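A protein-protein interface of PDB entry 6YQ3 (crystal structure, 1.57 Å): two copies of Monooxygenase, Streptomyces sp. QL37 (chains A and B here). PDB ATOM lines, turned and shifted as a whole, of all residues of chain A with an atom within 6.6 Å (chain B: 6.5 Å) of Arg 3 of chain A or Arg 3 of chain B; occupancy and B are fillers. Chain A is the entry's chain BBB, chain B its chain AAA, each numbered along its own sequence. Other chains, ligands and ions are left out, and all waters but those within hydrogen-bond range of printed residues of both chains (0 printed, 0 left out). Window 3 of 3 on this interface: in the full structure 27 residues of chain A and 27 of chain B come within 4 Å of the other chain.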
ATOM      1  N   SER A   2       6.436 -13.451  15.949  1.00  0.00           N
ATOM      2  CA  SER A   2       5.761 -12.281  15.389  1.00  0.00           C
ATOM      3  C   SER A   2       5.532 -12.467  13.885  1.00  0.00           C
ATOM      4  O   SER A   2       5.664 -11.537  13.103  1.00  0.00           O
ATOM      5  CB  SER A   2       6.497 -11.021  15.686  1.00  0.00           C
ATOM      6  OG  SER A   2       7.367 -10.655  14.611  1.00  0.00           O
ATOM      7  N   ARG A   3       4.988 -13.610  13.535  1.00  0.00           N
ATOM      8  CA  ARG A   3       4.723 -13.912  12.113  1.00  0.00           C
ATOM      9  C   ARG A   3       3.523 -13.133  11.558  1.00  0.00           C
ATOM     10  O   ARG A   3       3.335 -13.121  10.333  1.00  0.00           O
ATOM     11  CB  ARG A   3       4.525 -15.414  11.999  1.00  0.00           C
ATOM     12  CG  ARG A   3       5.800 -16.186  12.269  1.00  0.00           C
ATOM     13  CD  ARG A   3       5.564 -17.679  12.266  1.00  0.00           C
ATOM     14  NE  ARG A   3       4.841 -18.128  13.427  1.00  0.00           N
ATOM     15  CZ  ARG A   3       4.503 -19.390  13.671  1.00  0.00           C
ATOM     16  NH1 ARG A   3       3.845 -19.707  14.780  1.00  0.00           N
ATOM     17  NH2 ARG A   3       4.708 -20.311  12.747  1.00  0.00           N
ATOM     18  N   LEU A   4       2.659 -12.598  12.416  1.00  0.00           N
ATOM     19  CA  LEU A   4       1.409 -11.945  11.958  1.00  0.00           C
ATOM     20  C   LEU A   4       1.399 -10.453  12.330  1.00  0.00           C
ATOM     21  O   LEU A   4       0.327  -9.859  12.358  1.00  0.00           O
ATOM     22  CB  LEU A   4       0.191 -12.662  12.563  1.00  0.00           C
ATOM     23  CG  LEU A   4       0.091 -14.141  12.174  1.00  0.00           C
ATOM     24  CD1 LEU A   4      -1.112 -14.762  12.825  1.00  0.00           C
ATOM     25  CD2 LEU A   4       0.041 -14.323  10.629  1.00  0.00           C
ATOM     26  N   THR A   5       2.581  -9.844  12.546  1.00  0.00           N
ATOM     27  CA  THR A   5       2.674  -8.380  12.771  1.00  0.00           C
ATOM     28  C   THR A   5       1.951  -7.643  11.649  1.00  0.00           C
ATOM     29  O   THR A   5       2.142  -8.011  10.447  1.00  0.00           O
ATOM     30  CB  THR A   5       4.151  -7.977  12.863  1.00  0.00           C
ATOM     31  OG1 THR A   5       4.649  -8.706  13.997  1.00  0.00           O
ATOM     32  CG2 THR A   5       4.283  -6.485  13.011  1.00  0.00           C
ATOM     33  N   LYS A   7      -1.203  -7.759  10.857  1.00  0.00           N
ATOM     34  CA  LYS A   7      -2.346  -8.488  10.276  1.00  0.00           C
ATOM     35  C   LYS A   7      -3.541  -8.374  11.189  1.00  0.00           C
ATOM     36  O   LYS A   7      -3.386  -8.260  12.385  1.00  0.00           O
ATOM     37  CB  LYS A   7      -2.024  -9.975  10.026  1.00  0.00           C
ATOM     38  CG  LYS A   7      -0.779 -10.191   9.158  1.00  0.00           C
ATOM     39  CD  LYS A   7      -1.023  -9.852   7.719  1.00  0.00           C
ATOM     40  CE  LYS A   7      -0.155 -10.652   6.762  1.00  0.00           C
ATOM     41  NZ  LYS A   7       1.142 -10.048   6.713  1.00  0.00           N
ATOM     42  N   ARG A  28      -0.664 -13.599  19.885  1.00  0.00           N
ATOM     43  CA  ARG A  28       0.751 -13.762  20.318  1.00  0.00           C
ATOM     44  C   ARG A  28       1.653 -13.595  19.113  1.00  0.00           C
ATOM     45  O   ARG A  28       2.781 -13.129  19.318  1.00  0.00           O
ATOM     46  CB  ARG A  28       0.980 -15.138  20.915  1.00  0.00           C
ATOM     47  CG  ARG A  28       0.364 -15.404  22.270  1.00  0.00           C
ATOM     48  CD  ARG A  28       0.660 -16.836  22.658  1.00  0.00           C
ATOM     49  NE  ARG A  28      -0.005 -17.069  23.896  1.00  0.00           N
ATOM     50  CZ  ARG A  28      -0.186 -18.240  24.465  1.00  0.00           C
ATOM     51  NH1 ARG A  28       0.216 -19.363  23.874  1.00  0.00           N
ATOM     52  NH2 ARG A  28      -0.788 -18.276  25.637  1.00  0.00           N
ATOM     53  N   GLU A  29       1.202 -13.907  17.884  1.00  0.00           N
ATOM     54  CA  GLU A  29       2.032 -13.708  16.680  1.00  0.00           C
ATOM     55  C   GLU A  29       1.937 -12.272  16.163  1.00  0.00           C
ATOM     56  O   GLU A  29       2.533 -11.976  15.088  1.00  0.00           O
ATOM     57  CB  GLU A  29       1.526 -14.636  15.589  1.00  0.00           C
ATOM     58  CG  GLU A  29       1.690 -16.084  15.905  1.00  0.00           C
ATOM     59  CD  GLU A  29       3.105 -16.587  15.934  1.00  0.00           C
ATOM     60  OE1 GLU A  29       3.986 -16.025  15.263  1.00  0.00           O
ATOM     61  OE2 GLU A  29       3.310 -17.575  16.661  1.00  0.00           O
ATOM     62  N   GLY A  30       1.123 -11.426  16.798  1.00  0.00           N
ATOM     63  CA  GLY A  30       1.057 -10.004  16.461  1.00  0.00           C
ATOM     64  C   GLY A  30      -0.213  -9.599  15.786  1.00  0.00           C
ATOM     65  O   GLY A  30      -0.363  -8.402  15.451  1.00  0.00           O
ATOM     66  N   ASP A 228      -2.663 -24.530  17.499  1.00  0.00           N
ATOM     67  CA  ASP A 228      -1.303 -24.421  16.977  1.00  0.00           C
ATOM     68  C   ASP A 228      -1.291 -24.669  15.473  1.00  0.00           C
ATOM     69  O   ASP A 228      -0.497 -24.030  14.720  1.00  0.00           O
ATOM     70  CB  ASP A 228      -0.325 -25.322  17.718  1.00  0.00           C
ATOM     71  CG  ASP A 228       0.068 -24.811  19.076  1.00  0.00           C
ATOM     72  OD1 ASP A 228       0.027 -23.573  19.290  1.00  0.00           O
ATOM     73  OD2 ASP A 228       0.516 -25.688  19.878  1.00  0.00           O
ATOM     74  N   THR A 231      -2.951 -21.724  13.626  1.00  0.00           N
ATOM     75  CA  THR A 231      -2.018 -20.593  13.650  1.00  0.00           C
ATOM     76  C   THR A 231      -1.005 -20.765  12.522  1.00  0.00           C
ATOM     77  O   THR A 231      -0.718 -19.799  11.787  1.00  0.00           O
ATOM     78  CB  THR A 231      -1.337 -20.463  15.013  1.00  0.00           C
ATOM     79  OG1 THR A 231      -2.366 -20.159  15.942  1.00  0.00           O
ATOM     80  CG2 THR A 231      -0.290 -19.359  15.028  1.00  0.00           C
ATOM     81  N   PHE A 232      -0.425 -21.964  12.354  1.00  0.00           N
ATOM     82  CA  PHE A 232       0.529 -22.198  11.254  1.00  0.00           C
ATOM     83  C   PHE A 232      -0.150 -21.891   9.901  1.00  0.00           C
ATOM     84  O   PHE A 232       0.458 -21.217   9.038  1.00  0.00           O
ATOM     85  CB  PHE A 232       1.069 -23.618  11.279  1.00  0.00           C
ATOM     86  CG  PHE A 232       1.739 -23.938   9.972  1.00  0.00           C
ATOM     87  CD1 PHE A 232       2.954 -23.357   9.649  1.00  0.00           C
ATOM     88  CD2 PHE A 232       1.115 -24.790   9.055  1.00  0.00           C
ATOM     89  CE1 PHE A 232       3.516 -23.587   8.387  1.00  0.00           C
ATOM     90  CE2 PHE A 232       1.704 -25.021   7.822  1.00  0.00           C
ATOM     91  CZ  PHE A 232       2.873 -24.412   7.498  1.00  0.00           C
ATOM     92  N   ALA A 234      -2.464 -19.902   9.236  1.00  0.00           N
ATOM     93  CA  ALA A 234      -2.615 -18.427   9.106  1.00  0.00           C
ATOM     94  C   ALA A 234      -1.315 -17.687   8.703  1.00  0.00           C
ATOM     95  O   ALA A 234      -1.416 -16.562   8.246  1.00  0.00           O
ATOM     96  CB  ALA A 234      -3.099 -17.837  10.421  1.00  0.00           C
ATOM     97  N   THR A 235      -0.152 -18.348   8.793  1.00  0.00           N
ATOM     98  CA  THR A 235       1.144 -17.725   8.486  1.00  0.00           C
ATOM     99  C   THR A 235       1.529 -17.775   7.014  1.00  0.00           C
ATOM    100  O   THR A 235       0.949 -18.556   6.217  1.00  0.00           O
ATOM    101  CB  THR A 235       2.274 -18.245   9.362  1.00  0.00           C
ATOM    102  OG1 THR A 235       2.569 -19.591   8.966  1.00  0.00           O
ATOM    103  CG2 THR A 235       1.922 -18.104  10.820  1.00  0.00           C
ATOM    104  N   ASP A 236       2.561 -17.038   6.664  1.00  0.00           N
ATOM    105  CA  ASP A 236       3.062 -16.989   5.270  1.00  0.00           C
ATOM    106  C   ASP A 236       3.580 -18.379   4.839  1.00  0.00           C
ATOM    107  O   ASP A 236       3.405 -18.717   3.653  1.00  0.00           O
ATOM    108  CB  ASP A 236       4.207 -15.984   5.131  1.00  0.00           C
ATOM    109  CG  ASP A 236       4.809 -15.954   3.740  1.00  0.00           C
ATOM    110  OD1 ASP A 236       4.071 -15.832   2.805  1.00  0.00           O
ATOM    111  OD2 ASP A 236       5.993 -16.214   3.605  1.00  0.00           O
ATOM    112  N   GLU A 237       4.140 -19.171   5.758  1.00  0.00           N
ATOM    113  CA  GLU A 237       4.856 -20.419   5.424  1.00  0.00           C
ATOM    114  C   GLU A 237       3.881 -21.506   4.960  1.00  0.00           C
ATOM    115  O   GLU A 237       4.355 -22.519   4.479  1.00  0.00           O
ATOM    116  CB  GLU A 237       5.721 -20.907   6.597  1.00  0.00           C
ATOM    117  CG  GLU A 237       7.013 -20.097   6.738  1.00  0.00           C
ATOM    118  CD  GLU A 237       6.848 -18.666   7.214  1.00  0.00           C
ATOM    119  OE1 GLU A 237       5.952 -18.387   8.000  1.00  0.00           O
ATOM    120  OE2 GLU A 237       7.575 -17.787   6.651  1.00  0.00           O
ATOM    121  N   SER B   2      14.230 -20.416  16.264  1.00  0.00           N
ATOM    122  CA  SER B   2      15.012 -21.422  17.049  1.00  0.00           C
ATOM    123  C   SER B   2      14.067 -22.480  17.576  1.00  0.00           C
ATOM    124  O   SER B   2      14.285 -23.024  18.668  1.00  0.00           O
ATOM    125  CB  SER B   2      15.752 -20.807  18.153  1.00  0.00           C
ATOM    126  OG  SER B   2      16.504 -19.744  17.625  1.00  0.00           O
ATOM    127  N   ARG B   3      13.171 -22.919  16.719  1.00  0.00           N
ATOM    128  CA  ARG B   3      12.216 -23.969  17.139  1.00  0.00           C
ATOM    129  C   ARG B   3      12.866 -25.336  17.254  1.00  0.00           C
ATOM    130  O   ARG B   3      12.200 -26.221  17.840  1.00  0.00           O
ATOM    131  CB  ARG B   3      11.058 -24.003  16.142  1.00  0.00           C
ATOM    132  CG  ARG B   3      10.118 -22.823  16.303  1.00  0.00           C
ATOM    133  CD  ARG B   3       9.067 -22.836  15.220  1.00  0.00           C
ATOM    134  NE  ARG B   3       9.584 -22.509  13.900  1.00  0.00           N
ATOM    135  CZ  ARG B   3       8.880 -22.562  12.769  1.00  0.00           C
ATOM    136  NH1 ARG B   3       9.450 -22.342  11.606  1.00  0.00           N
ATOM    137  NH2 ARG B   3       7.586 -22.837  12.785  1.00  0.00           N
ATOM    138  N   LEU B   4      14.029 -25.544  16.678  1.00  0.00           N
ATOM    139  CA  LEU B   4      14.665 -26.890  16.639  1.00  0.00           C
ATOM    140  C   LEU B   4      16.037 -26.862  17.310  1.00  0.00           C
ATOM    141  O   LEU B   4      16.858 -27.765  17.060  1.00  0.00           O
ATOM    142  CB  LEU B   4      14.765 -27.385  15.196  1.00  0.00           C
ATOM    143  CG  LEU B   4      13.409 -27.534  14.485  1.00  0.00           C
ATOM    144  CD1 LEU B   4      13.678 -27.972  13.048  1.00  0.00           C
ATOM    145  CD2 LEU B   4      12.471 -28.484  15.273  1.00  0.00           C
ATOM    146  N   THR B   5      16.265 -25.901  18.234  1.00  0.00           N
ATOM    147  CA  THR B   5      17.516 -25.887  19.030  1.00  0.00           C
ATOM    148  C   THR B   5      17.719 -27.234  19.720  1.00  0.00           C
ATOM    149  O   THR B   5      16.759 -27.761  20.260  1.00  0.00           O
ATOM    150  CB  THR B   5      17.433 -24.777  20.087  1.00  0.00           C
ATOM    151  OG1 THR B   5      17.332 -23.594  19.293  1.00  0.00           O
ATOM    152  CG2 THR B   5      18.657 -24.728  20.984  1.00  0.00           C
ATOM    153  N   LYS B   7      18.178 -30.110  18.424  1.00  0.00           N
ATOM    154  CA  LYS B   7      17.684 -31.303  17.698  1.00  0.00           C
ATOM    155  C   LYS B   7      18.667 -31.694  16.607  1.00  0.00           C
ATOM    156  O   LYS B   7      19.297 -30.826  16.008  1.00  0.00           O
ATOM    157  CB  LYS B   7      16.329 -31.056  17.043  1.00  0.00           C
ATOM    158  CG  LYS B   7      15.303 -30.495  18.005  1.00  0.00           C
ATOM    159  CD  LYS B   7      14.725 -31.526  18.832  1.00  0.00           C
ATOM    160  CE  LYS B   7      13.370 -31.062  19.300  1.00  0.00           C
ATOM    161  NZ  LYS B   7      13.159 -31.746  20.568  1.00  0.00           N
ATOM    162  N   ARG B  28      18.281 -23.378   9.964  1.00  0.00           N
ATOM    163  CA  ARG B  28      17.939 -21.991  10.401  1.00  0.00           C
ATOM    164  C   ARG B  28      17.194 -22.048  11.738  1.00  0.00           C
ATOM    165  O   ARG B  28      17.308 -21.116  12.512  1.00  0.00           O
ATOM    166  CB  ARG B  28      17.065 -21.282   9.368  1.00  0.00           C
ATOM    167  CG  ARG B  28      17.797 -20.954   8.085  1.00  0.00           C
ATOM    168  CD  ARG B  28      16.781 -20.374   7.129  1.00  0.00           C
ATOM    169  NE  ARG B  28      17.493 -20.020   5.948  1.00  0.00           N
ATOM    170  CZ  ARG B  28      16.950 -19.699   4.791  1.00  0.00           C
ATOM    171  NH1 ARG B  28      15.639 -19.661   4.658  1.00  0.00           N
ATOM    172  NH2 ARG B  28      17.744 -19.373   3.789  1.00  0.00           N
ATOM    173  N   GLU B  29      16.426 -23.086  12.016  1.00  0.00           N
ATOM    174  CA  GLU B  29      15.665 -23.262  13.259  1.00  0.00           C
ATOM    175  C   GLU B  29      16.544 -23.870  14.349  1.00  0.00           C
ATOM    176  O   GLU B  29      16.037 -24.097  15.457  1.00  0.00           O
ATOM    177  CB  GLU B  29      14.506 -24.225  13.000  1.00  0.00           C
ATOM    178  CG  GLU B  29      13.527 -23.667  11.985  1.00  0.00           C
ATOM    179  CD  GLU B  29      12.742 -22.471  12.410  1.00  0.00           C
ATOM    180  OE1 GLU B  29      12.517 -22.258  13.626  1.00  0.00           O
ATOM    181  OE2 GLU B  29      12.276 -21.808  11.492  1.00  0.00           O
ATOM    182  N   GLY B  30      17.809 -24.149  14.048  1.00  0.00           N
ATOM    183  CA  GLY B  30      18.783 -24.589  15.051  1.00  0.00           C
ATOM    184  C   GLY B  30      19.071 -26.067  15.017  1.00  0.00           C
ATOM    185  O   GLY B  30      19.840 -26.539  15.844  1.00  0.00           O
ATOM    186  N   ASP B 228       9.149 -25.195   3.504  1.00  0.00           N
ATOM    187  CA  ASP B 228       8.544 -24.446   4.635  1.00  0.00           C
ATOM    188  C   ASP B 228       7.518 -25.365   5.301  1.00  0.00           C
ATOM    189  O   ASP B 228       7.340 -25.307   6.553  1.00  0.00           O
ATOM    190  CB  ASP B 228       7.867 -23.152   4.154  1.00  0.00           C
ATOM    191  CG  ASP B 228       8.883 -22.066   3.845  1.00  0.00           C
ATOM    192  OD1 ASP B 228      10.016 -22.090   4.464  1.00  0.00           O
ATOM    193  OD2 ASP B 228       8.520 -21.158   3.049  1.00  0.00           O
ATOM    194  N   THR B 231       9.355 -28.129   7.279  1.00  0.00           N
ATOM    195  CA  THR B 231       9.941 -27.515   8.496  1.00  0.00           C
ATOM    196  C   THR B 231       8.863 -27.380   9.562  1.00  0.00           C
ATOM    197  O   THR B 231       9.137 -27.737  10.740  1.00  0.00           O
ATOM    198  CB  THR B 231      10.568 -26.165   8.139  1.00  0.00           C
ATOM    199  OG1 THR B 231      11.618 -26.446   7.234  1.00  0.00           O
ATOM    200  CG2 THR B 231      11.103 -25.491   9.392  1.00  0.00           C
ATOM    201  N   PHE B 232       7.657 -26.894   9.219  1.00  0.00           N
ATOM    202  CA  PHE B 232       6.587 -26.816  10.219  1.00  0.00           C
ATOM    203  C   PHE B 232       6.284 -28.196  10.815  1.00  0.00           C
ATOM    204  O   PHE B 232       6.192 -28.373  12.056  1.00  0.00           O
ATOM    205  CB  PHE B 232       5.319 -26.192   9.637  1.00  0.00           C
ATOM    206  CG  PHE B 232       4.149 -26.462  10.567  1.00  0.00           C
ATOM    207  CD1 PHE B 232       4.019 -25.812  11.786  1.00  0.00           C
ATOM    208  CD2 PHE B 232       3.182 -27.380  10.200  1.00  0.00           C
ATOM    209  CE1 PHE B 232       2.969 -26.128  12.621  1.00  0.00           C
ATOM    210  CE2 PHE B 232       2.144 -27.684  11.049  1.00  0.00           C
ATOM    211  CZ  PHE B 232       2.063 -27.100  12.253  1.00  0.00           C
ATOM    212  N   ALA B 234       8.210 -30.650  11.167  1.00  0.00           N
ATOM    213  CA  ALA B 234       9.343 -31.037  12.045  1.00  0.00           C
ATOM    214  C   ALA B 234       9.285 -30.381  13.433  1.00  0.00           C
ATOM    215  O   ALA B 234       9.996 -30.842  14.350  1.00  0.00           O
ATOM    216  CB  ALA B 234      10.682 -30.705  11.393  1.00  0.00           C
ATOM    217  N   THR B 235       8.474 -29.329  13.620  1.00  0.00           N
ATOM    218  CA  THR B 235       8.423 -28.568  14.904  1.00  0.00           C
ATOM    219  C   THR B 235       7.435 -29.157  15.907  1.00  0.00           C
ATOM    220  O   THR B 235       6.589 -30.030  15.579  1.00  0.00           O
ATOM    221  CB  THR B 235       8.093 -27.091  14.652  1.00  0.00           C
ATOM    222  OG1 THR B 235       6.726 -26.902  14.284  1.00  0.00           O
ATOM    223  CG2 THR B 235       9.081 -26.507  13.652  1.00  0.00           C
ATOM    224  N   ASP B 236       7.509 -28.716  17.173  1.00  0.00           N
ATOM    225  CA  ASP B 236       6.620 -29.204  18.240  1.00  0.00           C
ATOM    226  C   ASP B 236       5.154 -28.856  17.946  1.00  0.00           C
ATOM    227  O   ASP B 236       4.274 -29.646  18.309  1.00  0.00           O
ATOM    228  CB  ASP B 236       7.027 -28.545  19.560  1.00  0.00           C
ATOM    229  CG  ASP B 236       6.058 -28.856  20.698  1.00  0.00           C
ATOM    230  OD1 ASP B 236       5.904 -30.030  20.988  1.00  0.00           O
ATOM    231  OD2 ASP B 236       5.442 -27.970  21.295  1.00  0.00           O
ATOM    232  N   GLU B 237       4.870 -27.775  17.202  1.00  0.00           N
ATOM    233  CA  GLU B 237       3.494 -27.273  17.021  1.00  0.00           C
ATOM    234  C   GLU B 237       2.690 -28.165  16.082  1.00  0.00           C
ATOM    235  O   GLU B 237       1.491 -27.973  16.017  1.00  0.00           O
ATOM    236  CB  GLU B 237       3.485 -25.820  16.544  1.00  0.00           C
ATOM    237  CG  GLU B 237       3.803 -24.840  17.663  1.00  0.00           C
ATOM    238  CD  GLU B 237       5.227 -24.820  18.181  1.00  0.00           C
ATOM    239  OE1 GLU B 237       6.219 -25.077  17.459  1.00  0.00           O
ATOM    240  OE2 GLU B 237       5.321 -24.660  19.436  1.00  0.00           O
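OG1 of Thr 235 of chain A lies within hydrogen-bond range of O of Phe 232 of chain A (2.7 Å). The guanidinium group of Arg 3 of chain A lies within salt-bridge range of the side-chain carboxylate of Glu 29 of chain A (2.9 Å). The guanidinium group (NH1) of Arg 3 of chain B is in salt-bridge range of the side-chain carboxylate (OE2) of Glu 29 of chain B (2.9 Å). The side-chain hydroxyl (OG1) of Thr 235 of chain B lies within hydrogen-bond range of the backbone carbonyl oxygen (O) of Phe 232 of chain B.
NH2 of Arg 3 of chain A touches NH2 of Arg 3 of chain B (3.8 Å). Glu 237 of chain B touches Asp 228 of chain A (O to CB, 3.6 Å). Phe 232 of chain B touches Phe 232 of chain A. Glu 237 of chain A touches Asp 228 of chain B (O to CB, 3.6 Å).
Arg 3 of chain A touches one residue of chain B. Of the printed residues of chain B, Asp 228 of chain A touches Glu 237. Of the printed residues of chain B, Phe 232 of chain A touches Phe 232. Thr 235 of chain A touches none of the printed residues of chain B. Printed residues of chain B within 4 Å of Glu 237 of chain A: Asp 228. Of the printed residues of chain A, Arg 3 of chain B touches Arg 3. Of the printed residues of chain A, Glu 237 of chain B touches Asp 228 (3.6 Å). The nearest residue of chain A that does not touch Arg 3 of chain B is Phe 232 of chain A (5.6 Å). The nearest printed residue of chain B that does not touch Asp 228 of chain A is Phe 232 of chain B (4.6 Å).
Hydrophobic or aromatic side chains of chain A within 4 Å of the printed part of chain B: Phe 232. Hydrophobic or aromatic side chains of chain B that line the printed part of chain A: Phe 232.
Arg 3 of chain A touches its own counterpart, Arg 3 of chain B. Asp 228 of chain A touches Glu 237 of chain B, and with the chains exchanged Glu 237 of chain A touches Asp 228 of chain B. Phe 232 of chain A touches its own counterpart, Phe 232 of chain B. Of the 4 pairs that touch across the chains among the printed residues, 4 have their exchanged pair printed and touching as well.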
